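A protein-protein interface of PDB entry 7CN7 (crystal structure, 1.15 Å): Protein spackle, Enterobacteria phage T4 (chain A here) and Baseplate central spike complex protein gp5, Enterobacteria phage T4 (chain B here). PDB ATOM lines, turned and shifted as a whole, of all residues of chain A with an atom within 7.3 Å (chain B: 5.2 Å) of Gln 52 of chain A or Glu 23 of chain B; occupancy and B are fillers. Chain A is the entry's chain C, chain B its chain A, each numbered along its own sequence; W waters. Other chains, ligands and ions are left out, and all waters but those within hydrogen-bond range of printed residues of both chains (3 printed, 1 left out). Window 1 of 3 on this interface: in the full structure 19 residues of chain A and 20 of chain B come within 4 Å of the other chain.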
ATOM      1  N   GLU A  19     -23.601 -18.278  -5.967  1.00  0.00           N
ATOM      2  CA  GLU A  19     -23.396 -16.881  -5.622  1.00  0.00           C
ATOM      3  C   GLU A  19     -24.633 -16.281  -4.969  1.00  0.00           C
ATOM      4  O   GLU A  19     -24.516 -15.465  -4.047  1.00  0.00           O
ATOM      5  CB  GLU A  19     -22.940 -16.112  -6.850  1.00  0.00           C
ATOM      6  CG  GLU A  19     -21.521 -16.596  -7.207  1.00  0.00           C
ATOM      7  CD  GLU A  19     -20.797 -15.873  -8.286  1.00  0.00           C
ATOM      8  OE1 GLU A  19     -21.392 -15.108  -9.029  1.00  0.00           O
ATOM      9  OE2 GLU A  19     -19.588 -16.105  -8.452  1.00  0.00           O
ATOM     10  N   ILE A  22     -24.357 -17.486  -1.327  1.00  0.00           N
ATOM     11  CA  ILE A  22     -23.293 -16.796  -0.604  1.00  0.00           C
ATOM     12  C   ILE A  22     -23.722 -15.371  -0.287  1.00  0.00           C
ATOM     13  O   ILE A  22     -23.563 -14.882   0.842  1.00  0.00           O
ATOM     14  CB  ILE A  22     -21.980 -16.809  -1.416  1.00  0.00           C
ATOM     15  CG1 ILE A  22     -21.405 -18.227  -1.468  1.00  0.00           C
ATOM     16  CG2 ILE A  22     -20.968 -15.839  -0.804  1.00  0.00           C
ATOM     17  CD1 ILE A  22     -20.264 -18.389  -2.437  1.00  0.00           C
ATOM     18  N   GLN A  44     -18.729  -4.135  -2.961  1.00  0.00           N
ATOM     19  CA  GLN A  44     -17.522  -4.959  -3.010  1.00  0.00           C
ATOM     20  C   GLN A  44     -17.795  -6.368  -3.531  1.00  0.00           C
ATOM     21  O   GLN A  44     -16.926  -6.963  -4.175  1.00  0.00           O
ATOM     22  CB  GLN A  44     -16.877  -5.027  -1.628  1.00  0.00           C
ATOM     23  CG  GLN A  44     -16.110  -3.779  -1.263  1.00  0.00           C
ATOM     24  CD  GLN A  44     -14.960  -3.529  -2.210  1.00  0.00           C
ATOM     25  OE1 GLN A  44     -14.184  -4.438  -2.524  1.00  0.00           O
ATOM     26  NE2 GLN A  44     -14.841  -2.310  -2.684  1.00  0.00           N
ATOM     27  N   LEU A  45     -18.976  -6.922  -3.287  1.00  0.00           N
ATOM     28  CA  LEU A  45     -19.329  -8.181  -3.923  1.00  0.00           C
ATOM     29  C   LEU A  45     -19.410  -8.019  -5.433  1.00  0.00           C
ATOM     30  O   LEU A  45     -18.987  -8.903  -6.182  1.00  0.00           O
ATOM     31  CB  LEU A  45     -20.630  -8.723  -3.338  1.00  0.00           C
ATOM     32  CG  LEU A  45     -20.554  -9.130  -1.864  1.00  0.00           C
ATOM     33  CD1 LEU A  45     -21.920  -9.641  -1.397  1.00  0.00           C
ATOM     34  CD2 LEU A  45     -19.488 -10.162  -1.588  1.00  0.00           C
ATOM     35  N   SER A  47     -17.806  -5.592  -7.332  1.00  0.00           N
ATOM     36  CA  SER A  47     -16.520  -5.272  -7.925  1.00  0.00           C
ATOM     37  C   SER A  47     -15.515  -6.395  -7.765  1.00  0.00           C
ATOM     38  O   SER A  47     -14.682  -6.599  -8.646  1.00  0.00           O
ATOM     39  CB  SER A  47     -15.932  -3.989  -7.322  1.00  0.00           C
ATOM     40  OG  SER A  47     -15.694  -4.084  -5.928  1.00  0.00           O
ATOM     41  N   GLY A  48     -15.572  -7.105  -6.653  1.00  0.00           N
ATOM     42  CA  GLY A  48     -14.545  -8.063  -6.283  1.00  0.00           C
ATOM     43  C   GLY A  48     -14.918  -9.512  -6.475  1.00  0.00           C
ATOM     44  O   GLY A  48     -14.037 -10.368  -6.462  1.00  0.00           O
ATOM     45  N   GLY A  49     -16.200  -9.805  -6.650  1.00  0.00           N
ATOM     46  CA  GLY A  49     -16.678 -11.160  -6.818  1.00  0.00           C
ATOM     47  C   GLY A  49     -17.271 -11.739  -5.547  1.00  0.00           C
ATOM     48  O   GLY A  49     -17.105 -11.225  -4.436  1.00  0.00           O
ATOM     49  N   VAL A  50     -17.966 -12.854  -5.738  1.00  0.00           N
ATOM     50  CA  VAL A  50     -18.697 -13.535  -4.685  1.00  0.00           C
ATOM     51  C   VAL A  50     -18.164 -14.939  -4.412  1.00  0.00           C
ATOM     52  O   VAL A  50     -18.109 -15.377  -3.256  1.00  0.00           O
ATOM     53  CB  VAL A  50     -20.208 -13.587  -5.039  1.00  0.00           C
ATOM     54  CG1 VAL A  50     -20.977 -14.429  -4.029  1.00  0.00           C
ATOM     55  CG2 VAL A  50     -20.784 -12.190  -5.119  1.00  0.00           C
ATOM     56  N   MET A  51     -17.806 -15.681  -5.459  1.00  0.00           N
ATOM     57  CA  MET A  51     -17.544 -17.108  -5.311  1.00  0.00           C
ATOM     58  C   MET A  51     -16.416 -17.398  -4.338  1.00  0.00           C
ATOM     59  O   MET A  51     -16.426 -18.446  -3.686  1.00  0.00           O
ATOM     60  CB  MET A  51     -17.202 -17.735  -6.667  1.00  0.00           C
ATOM     61  CG  MET A  51     -16.888 -19.207  -6.540  1.00  0.00           C
ATOM     62  SD  MET A  51     -18.328 -20.189  -6.030  1.00  0.00           S
ATOM     63  CE  MET A  51     -19.189 -20.196  -7.603  1.00  0.00           C
ATOM     64  N   GLN A  52     -15.415 -16.529  -4.257  1.00  0.00           N
ATOM     65  CA  GLN A  52     -14.230 -16.820  -3.465  1.00  0.00           C
ATOM     66  C   GLN A  52     -14.531 -17.044  -2.002  1.00  0.00           C
ATOM     67  O   GLN A  52     -13.714 -17.664  -1.329  1.00  0.00           O
ATOM     68  CB  GLN A  52     -13.170 -15.718  -3.598  1.00  0.00           C
ATOM     69  CG  GLN A  52     -13.589 -14.322  -3.146  1.00  0.00           C
ATOM     70  CD  GLN A  52     -14.076 -13.455  -4.282  1.00  0.00           C
ATOM     71  OE1 GLN A  52     -14.840 -13.909  -5.150  1.00  0.00           O
ATOM     72  NE2 GLN A  52     -13.685 -12.191  -4.266  1.00  0.00           N
ATOM     73  N   TYR A  53     -15.647 -16.534  -1.491  1.00  0.00           N
ATOM     74  CA  TYR A  53     -15.954 -16.650  -0.076  1.00  0.00           C
ATOM     75  C   TYR A  53     -16.516 -18.009   0.306  1.00  0.00           C
ATOM     76  O   TYR A  53     -16.806 -18.235   1.482  1.00  0.00           O
ATOM     77  CB  TYR A  53     -16.897 -15.522   0.375  1.00  0.00           C
ATOM     78  CG  TYR A  53     -16.311 -14.155   0.067  1.00  0.00           C
ATOM     79  CD1 TYR A  53     -15.158 -13.710   0.693  1.00  0.00           C
ATOM     80  CD2 TYR A  53     -16.857 -13.356  -0.914  1.00  0.00           C
ATOM     81  CE1 TYR A  53     -14.598 -12.489   0.370  1.00  0.00           C
ATOM     82  CE2 TYR A  53     -16.293 -12.148  -1.257  1.00  0.00           C
ATOM     83  CZ  TYR A  53     -15.172 -11.713  -0.602  1.00  0.00           C
ATOM     84  OH  TYR A  53     -14.587 -10.509  -0.909  1.00  0.00           O
ATOM     85  N   ASN A  54     -16.683 -18.932  -0.641  1.00  0.00           N
ATOM     86  CA  ASN A  54     -17.301 -20.201  -0.275  1.00  0.00           C
ATOM     87  C   ASN A  54     -16.491 -20.950   0.769  1.00  0.00           C
ATOM     88  O   ASN A  54     -17.057 -21.579   1.673  1.00  0.00           O
ATOM     89  CB  ASN A  54     -17.551 -21.084  -1.502  1.00  0.00           C
ATOM     90  CG  ASN A  54     -16.338 -21.840  -2.005  1.00  0.00           C
ATOM     91  OD1 ASN A  54     -15.273 -21.283  -2.255  1.00  0.00           O
ATOM     92  ND2 ASN A  54     -16.516 -23.145  -2.172  1.00  0.00           N
ATOM     93  N   TYR A  55     -15.162 -20.912   0.653  1.00  0.00           N
ATOM     94  CA  TYR A  55     -14.331 -21.742   1.515  1.00  0.00           C
ATOM     95  C   TYR A  55     -14.409 -21.281   2.961  1.00  0.00           C
ATOM     96  O   TYR A  55     -14.679 -22.088   3.862  1.00  0.00           O
ATOM     97  CB  TYR A  55     -12.889 -21.768   0.997  1.00  0.00           C
ATOM     98  CG  TYR A  55     -12.023 -22.669   1.829  1.00  0.00           C
ATOM     99  CD1 TYR A  55     -11.999 -24.042   1.612  1.00  0.00           C
ATOM    100  CD2 TYR A  55     -11.258 -22.153   2.875  1.00  0.00           C
ATOM    101  CE1 TYR A  55     -11.221 -24.878   2.423  1.00  0.00           C
ATOM    102  CE2 TYR A  55     -10.495 -22.956   3.673  1.00  0.00           C
ATOM    103  CZ  TYR A  55     -10.473 -24.313   3.437  1.00  0.00           C
ATOM    104  OH  TYR A  55      -9.701 -25.107   4.232  1.00  0.00           O
ATOM    105  N   VAL A  56     -14.208 -19.990   3.212  1.00  0.00           N
ATOM    106  CA  VAL A  56     -14.273 -19.522   4.592  1.00  0.00           C
ATOM    107  C   VAL A  56     -15.667 -19.676   5.173  1.00  0.00           C
ATOM    108  O   VAL A  56     -15.814 -19.967   6.363  1.00  0.00           O
ATOM    109  CB  VAL A  56     -13.775 -18.076   4.768  1.00  0.00           C
ATOM    110  CG1 VAL A  56     -12.274 -17.961   4.542  1.00  0.00           C
ATOM    111  CG2 VAL A  56     -14.537 -17.047   3.920  1.00  0.00           C
ATOM    112  N   LEU A  57     -16.721 -19.468   4.364  1.00  0.00           N
ATOM    113  CA  LEU A  57     -18.076 -19.482   4.916  1.00  0.00           C
ATOM    114  C   LEU A  57     -18.537 -20.881   5.256  1.00  0.00           C
ATOM    115  O   LEU A  57     -19.270 -21.072   6.236  1.00  0.00           O
ATOM    116  CB  LEU A  57     -19.067 -18.872   3.940  1.00  0.00           C
ATOM    117  CG  LEU A  57     -19.087 -17.368   3.874  1.00  0.00           C
ATOM    118  CD1 LEU A  57     -19.922 -16.920   2.692  1.00  0.00           C
ATOM    119  CD2 LEU A  57     -19.607 -16.767   5.191  1.00  0.00           C
ATOM    120  N   GLU A  71     -13.997  -9.484   6.030  1.00  0.00           N
ATOM    121  CA  GLU A  71     -13.378 -10.204   4.933  1.00  0.00           C
ATOM    122  C   GLU A  71     -13.677  -9.531   3.610  1.00  0.00           C
ATOM    123  O   GLU A  71     -12.813  -9.468   2.729  1.00  0.00           O
ATOM    124  CB  GLU A  71     -13.861 -11.656   4.919  1.00  0.00           C
ATOM    125  CG  GLU A  71     -12.991 -12.584   4.096  1.00  0.00           C
ATOM    126  CD  GLU A  71     -11.671 -12.959   4.746  1.00  0.00           C
ATOM    127  OE1 GLU A  71     -11.376 -12.474   5.854  1.00  0.00           O
ATOM    128  OE2 GLU A  71     -10.936 -13.749   4.109  1.00  0.00           O
ATOM    129  N   MET B  18      -3.557 -19.719   2.890  1.00  0.00           N
ATOM    130  CA  MET B  18      -3.866 -18.329   2.605  1.00  0.00           C
ATOM    131  C   MET B  18      -4.704 -18.187   1.349  1.00  0.00           C
ATOM    132  O   MET B  18      -5.628 -17.364   1.297  1.00  0.00           O
ATOM    133  CB  MET B  18      -2.546 -17.550   2.482  1.00  0.00           C
ATOM    134  CG  MET B  18      -2.727 -16.055   2.519  1.00  0.00           C
ATOM    135  SD  MET B  18      -1.169 -15.247   2.061  1.00  0.00           S
ATOM    136  CE  MET B  18      -1.381 -13.602   2.681  1.00  0.00           C
ATOM    137  N   LEU B  19      -4.378 -18.982   0.326  1.00  0.00           N
ATOM    138  CA  LEU B  19      -5.043 -18.861  -0.958  1.00  0.00           C
ATOM    139  C   LEU B  19      -6.358 -19.635  -1.013  1.00  0.00           C
ATOM    140  O   LEU B  19      -7.270 -19.195  -1.709  1.00  0.00           O
ATOM    141  CB  LEU B  19      -4.089 -19.221  -2.088  1.00  0.00           C
ATOM    142  CG  LEU B  19      -2.961 -18.194  -2.253  1.00  0.00           C
ATOM    143  CD1 LEU B  19      -1.863 -18.735  -3.170  1.00  0.00           C
ATOM    144  CD2 LEU B  19      -3.477 -16.871  -2.810  1.00  0.00           C
ATOM    145  N   ARG B  20      -6.512 -20.754  -0.297  1.00  0.00           N
ATOM    146  CA  ARG B  20      -7.864 -21.309  -0.166  1.00  0.00           C
ATOM    147  C   ARG B  20      -8.802 -20.260   0.426  1.00  0.00           C
ATOM    148  O   ARG B  20      -9.942 -20.094  -0.025  1.00  0.00           O
ATOM    149  CB  ARG B  20      -7.871 -22.548   0.743  1.00  0.00           C
ATOM    150  CG  ARG B  20      -7.395 -23.827   0.110  1.00  0.00           C
ATOM    151  CD  ARG B  20      -7.699 -25.059   0.950  1.00  0.00           C
ATOM    152  NE  ARG B  20      -6.929 -25.105   2.194  1.00  0.00           N
ATOM    153  CZ  ARG B  20      -5.738 -25.680   2.350  1.00  0.00           C
ATOM    154  NH1 ARG B  20      -5.136 -26.267   1.338  1.00  0.00           N
ATOM    155  NH2 ARG B  20      -5.145 -25.657   3.529  1.00  0.00           N
ATOM    156  N   ARG B  21      -8.325 -19.540   1.439  1.00  0.00           N
ATOM    157  CA  ARG B  21      -9.117 -18.487   2.054  1.00  0.00           C
ATOM    158  C   ARG B  21      -9.450 -17.367   1.071  1.00  0.00           C
ATOM    159  O   ARG B  21     -10.618 -16.979   0.937  1.00  0.00           O
ATOM    160  CB  ARG B  21      -8.389 -17.947   3.277  1.00  0.00           C
ATOM    161  CG  ARG B  21      -9.004 -16.656   3.796  1.00  0.00           C
ATOM    162  CD  ARG B  21      -8.563 -16.395   5.192  1.00  0.00           C
ATOM    163  NE  ARG B  21      -9.011 -15.106   5.679  1.00  0.00           N
ATOM    164  CZ  ARG B  21      -8.708 -14.633   6.874  1.00  0.00           C
ATOM    165  NH1 ARG B  21      -7.956 -15.334   7.709  1.00  0.00           N
ATOM    166  NH2 ARG B  21      -9.156 -13.438   7.232  1.00  0.00           N
ATOM    167  N   ASP B  22      -8.451 -16.857   0.346  1.00  0.00           N
ATOM    168  CA  ASP B  22      -8.683 -15.680  -0.476  1.00  0.00           C
ATOM    169  C   ASP B  22      -9.286 -15.996  -1.835  1.00  0.00           C
ATOM    170  O   ASP B  22      -9.985 -15.138  -2.388  1.00  0.00           O
ATOM    171  CB  ASP B  22      -7.383 -14.896  -0.667  1.00  0.00           C
ATOM    172  CG  ASP B  22      -6.984 -14.086   0.555  1.00  0.00           C
ATOM    173  OD1 ASP B  22      -7.822 -13.819   1.436  1.00  0.00           O
ATOM    174  OD2 ASP B  22      -5.800 -13.697   0.578  1.00  0.00           O
ATOM    175  N   GLU B  23      -9.021 -17.183  -2.383  1.00  0.00           N
ATOM    176  CA  GLU B  23      -9.465 -17.551  -3.718  1.00  0.00           C
ATOM    177  C   GLU B  23     -10.681 -18.470  -3.707  1.00  0.00           C
ATOM    178  O   GLU B  23     -11.333 -18.635  -4.753  1.00  0.00           O
ATOM    179  CB  GLU B  23      -8.360 -18.273  -4.506  1.00  0.00           C
ATOM    180  CG  GLU B  23      -7.074 -17.514  -4.682  1.00  0.00           C
ATOM    181  CD  GLU B  23      -7.124 -16.461  -5.773  1.00  0.00           C
ATOM    182  OE1 GLU B  23      -8.153 -16.406  -6.501  1.00  0.00           O
ATOM    183  OE2 GLU B  23      -6.180 -15.646  -5.882  1.00  0.00           O
ATOM    184  N   GLY B  24     -10.995 -19.072  -2.571  1.00  0.00           N
ATOM    185  CA  GLY B  24     -12.044 -20.071  -2.509  1.00  0.00           C
ATOM    186  C   GLY B  24     -11.604 -21.396  -3.099  1.00  0.00           C
ATOM    187  O   GLY B  24     -10.451 -21.588  -3.493  1.00  0.00           O
ATOM    188  N   LEU B  25     -12.568 -22.313  -3.187  1.00  0.00           N
ATOM    189  CA  LEU B  25     -12.273 -23.687  -3.581  1.00  0.00           C
ATOM    190  C   LEU B  25     -13.445 -24.208  -4.402  1.00  0.00           C
ATOM    191  O   LEU B  25     -14.537 -24.424  -3.870  1.00  0.00           O
ATOM    192  CB  LEU B  25     -11.996 -24.561  -2.363  1.00  0.00           C
ATOM    193  CG  LEU B  25     -11.203 -25.854  -2.580  1.00  0.00           C
ATOM    194  CD1 LEU B  25     -11.101 -26.595  -1.229  1.00  0.00           C
ATOM    195  CD2 LEU B  25     -11.811 -26.756  -3.613  1.00  0.00           C
ATOM    196  N   TYR B  30     -16.197 -22.242 -12.816  1.00  0.00           N
ATOM    197  CA  TYR B  30     -16.900 -20.987 -12.639  1.00  0.00           C
ATOM    198  C   TYR B  30     -16.138 -19.937 -13.424  1.00  0.00           C
ATOM    199  O   TYR B  30     -15.055 -20.199 -13.963  1.00  0.00           O
ATOM    200  CB  TYR B  30     -17.027 -20.609 -11.168  1.00  0.00           C
ATOM    201  CG  TYR B  30     -15.763 -20.174 -10.478  1.00  0.00           C
ATOM    202  CD1 TYR B  30     -14.805 -21.099 -10.097  1.00  0.00           C
ATOM    203  CD2 TYR B  30     -15.544 -18.841 -10.157  1.00  0.00           C
ATOM    204  CE1 TYR B  30     -13.643 -20.712  -9.424  1.00  0.00           C
ATOM    205  CE2 TYR B  30     -14.418 -18.446  -9.486  1.00  0.00           C
ATOM    206  CZ  TYR B  30     -13.475 -19.386  -9.102  1.00  0.00           C
ATOM    207  OH  TYR B  30     -12.366 -18.931  -8.422  1.00  0.00           O
ATOM    208  N   GLY B  40     -10.786 -24.952  -9.059  1.00  0.00           N
ATOM    209  CA  GLY B  40      -9.816 -25.188  -8.005  1.00  0.00           C
ATOM    210  C   GLY B  40      -9.672 -23.988  -7.099  1.00  0.00           C
ATOM    211  O   GLY B  40     -10.660 -23.346  -6.709  1.00  0.00           O
ATOM    212  N   ILE B  41      -8.418 -23.708  -6.739  1.00  0.00           N
ATOM    213  CA  ILE B  41      -8.021 -22.587  -5.900  1.00  0.00           C
ATOM    214  C   ILE B  41      -7.441 -21.540  -6.858  1.00  0.00           C
ATOM    215  O   ILE B  41      -6.219 -21.472  -7.078  1.00  0.00           O
ATOM    216  CB  ILE B  41      -7.024 -23.049  -4.821  1.00  0.00           C
ATOM    217  CG1 ILE B  41      -7.612 -24.152  -3.925  1.00  0.00           C
ATOM    218  CG2 ILE B  41      -6.649 -21.858  -3.958  1.00  0.00           C
ATOM    219  CD1 ILE B  41      -7.671 -25.567  -4.455  1.00  0.00           C
ATOM    220  N   GLY B  42      -8.310 -20.748  -7.472  1.00  0.00           N
ATOM    221  CA  GLY B  42      -7.871 -19.738  -8.402  1.00  0.00           C
ATOM    222  C   GLY B  42      -7.114 -20.222  -9.613  1.00  0.00           C
ATOM    223  O   GLY B  42      -6.298 -19.472 -10.163  1.00  0.00           O
ATOM    224  N   PHE B 121      -0.401 -14.166  -7.020  1.00  0.00           N
ATOM    225  CA  PHE B 121      -1.352 -15.205  -7.379  1.00  0.00           C
ATOM    226  C   PHE B 121      -2.631 -14.590  -7.942  1.00  0.00           C
ATOM    227  O   PHE B 121      -3.251 -15.153  -8.850  1.00  0.00           O
ATOM    228  CB  PHE B 121      -1.655 -16.091  -6.176  1.00  0.00           C
ATOM    229  CG  PHE B 121      -2.096 -17.483  -6.536  1.00  0.00           C
ATOM    230  CD1 PHE B 121      -1.154 -18.471  -6.795  1.00  0.00           C
ATOM    231  CD2 PHE B 121      -3.428 -17.801  -6.617  1.00  0.00           C
ATOM    232  CE1 PHE B 121      -1.544 -19.767  -7.097  1.00  0.00           C
ATOM    233  CE2 PHE B 121      -3.811 -19.084  -6.925  1.00  0.00           C
ATOM    234  CZ  PHE B 121      -2.882 -20.072  -7.172  1.00  0.00           C
ATOM    235  N   GLN B 122      -3.030 -13.433  -7.406  1.00  0.00           N
ATOM    236  CA  GLN B 122      -4.247 -12.752  -7.844  1.00  0.00           C
ATOM    237  C   GLN B 122      -4.082 -12.090  -9.206  1.00  0.00           C
ATOM    238  O   GLN B 122      -4.985 -12.166 -10.053  1.00  0.00           O
ATOM    239  CB  GLN B 122      -4.651 -11.695  -6.811  1.00  0.00           C
ATOM    240  CG  GLN B 122      -5.977 -11.035  -7.130  1.00  0.00           C
ATOM    241  CD  GLN B 122      -6.392 -10.014  -6.098  1.00  0.00           C
ATOM    242  OE1 GLN B 122      -5.710  -9.780  -5.119  1.00  0.00           O
ATOM    243  NE2 GLN B 122      -7.542  -9.397  -6.322  1.00  0.00           N
ATOM    244  N   ARG B 162      -9.558  -8.153   0.560  1.00  0.00           N
ATOM    245  CA  ARG B 162      -8.283  -8.823   0.361  1.00  0.00           C
ATOM    246  C   ARG B 162      -7.136  -7.827   0.370  1.00  0.00           C
ATOM    247  O   ARG B 162      -6.118  -8.048   1.027  1.00  0.00           O
ATOM    248  CB  ARG B 162      -8.325  -9.595  -0.954  1.00  0.00           C
ATOM    249  CG  ARG B 162      -7.094 -10.464  -1.200  1.00  0.00           C
ATOM    250  CD  ARG B 162      -7.327 -11.311  -2.422  1.00  0.00           C
ATOM    251  NE  ARG B 162      -6.200 -12.202  -2.710  1.00  0.00           N
ATOM    252  CZ  ARG B 162      -6.180 -13.081  -3.694  1.00  0.00           C
ATOM    253  NH1 ARG B 162      -7.225 -13.218  -4.476  1.00  0.00           N
ATOM    254  NH2 ARG B 162      -5.106 -13.834  -3.892  1.00  0.00           N
HETATM  255  O   HOH W   1     -13.000 -18.432   1.118  1.00  0.00           O
HETATM  256  O   HOH W   2      -7.297 -24.022   4.936  1.00  0.00           O
HETATM  257  O   HOH W   3     -11.864 -14.489   1.618  1.00  0.00           O
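O of Gln 52 of chain A lies close to N of Gly 24 of chain B, 3.3 Å away.
The guanidinium group of Arg 20 of chain B sits at hydrogen-bond distance from the side-chain hydroxyl of Tyr 55 of chain A, 3.4 Å away.
The side-chain amide nitrogen of Asn 54 of chain A is in hydrogen-bond range of the backbone carbonyl oxygen of Leu 25 of chain B, at 2.9 Å.
OE1 of Glu 71 of chain A lies within salt-bridge range of NH2 of Arg 21 of chain B (2.8 Å).
NH2 of Arg 162 of chain B lies within salt-bridge range of OE2 of Glu 23 of chain B, at 2.9 Å.
The backbone NH (N) of Val 50 of chain A sits at hydrogen-bond distance from the side-chain amide oxygen (OE1) of Gln 52 of chain A (3.4 Å).
The side-chain carboxylate (OD2) of Asp 22 of chain B is in salt-bridge range of the guanidinium group (NE) of Arg 162 of chain B, at 3.6 Å.
The side-chain amide oxygen (OD1) of Asn 54 of chain A lies close to the backbone carbonyl oxygen (O) of Met 51 of chain A.
The side-chain amide nitrogen (NE2) of Gln 52 of chain A sits at hydrogen-bond distance from the backbone carbonyl oxygen (O) of Gly 48 of chain A, at 2.9 Å.
CD2 of Tyr 30 of chain B touches CG of Met 51 of chain A, 3.9 Å away.
O of Arg 21 of chain B touches O of Gln 52 of chain A, at 3.9 Å.
O of Asp 22 of chain B touches CB of Gln 52 of chain A, at 3.5 Å.
Gln 52 of chain A touches Glu 23 of chain B.
Asn 54 of chain A touches Gly 24 of chain B (OD1 to CA, 3.5 Å).
Gly 24 of chain B touches Tyr 55 of chain A (CA to CB, 3.99 Å).
CD1 of Tyr 55 of chain A touches CD1 of Leu 25 of chain B, at 3.9 Å.
Val 56 of chain A touches Arg 21 of chain B (CG1 to CG, 3.6 Å).
Gln 52 of chain A touches just these residues of chain B: Arg 21, Asp 22, Glu 23 and Gly 24.
Of the printed residues of chain A, Glu 23 of chain B touches Gln 52 (3.6 Å).
Printed residues of chain B within 4 Å of Asn 54 of chain A: Gly 24 (3.5 Å) and Leu 25 (2.9 Å).
Of the printed residues of chain B, Val 56 of chain A touches Arg 21 (3.6 Å).
The nearest residue of chain B that does not touch Gln 52 of chain A is Arg 20 of chain B (4.7 Å).
The nearest printed residue of chain A that does not touch Glu 23 of chain B is Met 51 of chain A (5.2 Å).
Printed residues of chain A that touch a printed residue of chain B: Met 51, Gln 52, Asn 54, Tyr 55, Val 56 and Glu 71.
Hydrophobic or aromatic side chains of chain B within 4 Å of the printed part of chain A: Leu 25 and Tyr 30.
Among the printed residues, 12 pairs touch across the chains.
Among the printed residues, Asp or Glu carboxylates within 4 Å of a Lys or Arg side-chain nitrogen of the other chain: Glu 71 of chain A with Arg 21 of chain B.
Water W1 lies within hydrogen-bond range of O of Gln 52 of chain A (2.7 Å), O of Arg 21 of chain B (2.8 Å), N of Val 56 of chain A (2.9 Å) and N of Tyr 55 of chain A (3.3 Å).
Water W2 lies within hydrogen-bond range of OH of Tyr 55 of chain A (2.7 Å) and NE of Arg 20 of chain B (3.0 Å).
Water W3 lies within hydrogen-bond range of the side-chain carboxylate of Glu 71 of chain A (2.8 Å) and the backbone carbonyl oxygen of Arg 21 of chain B (2.9 Å).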
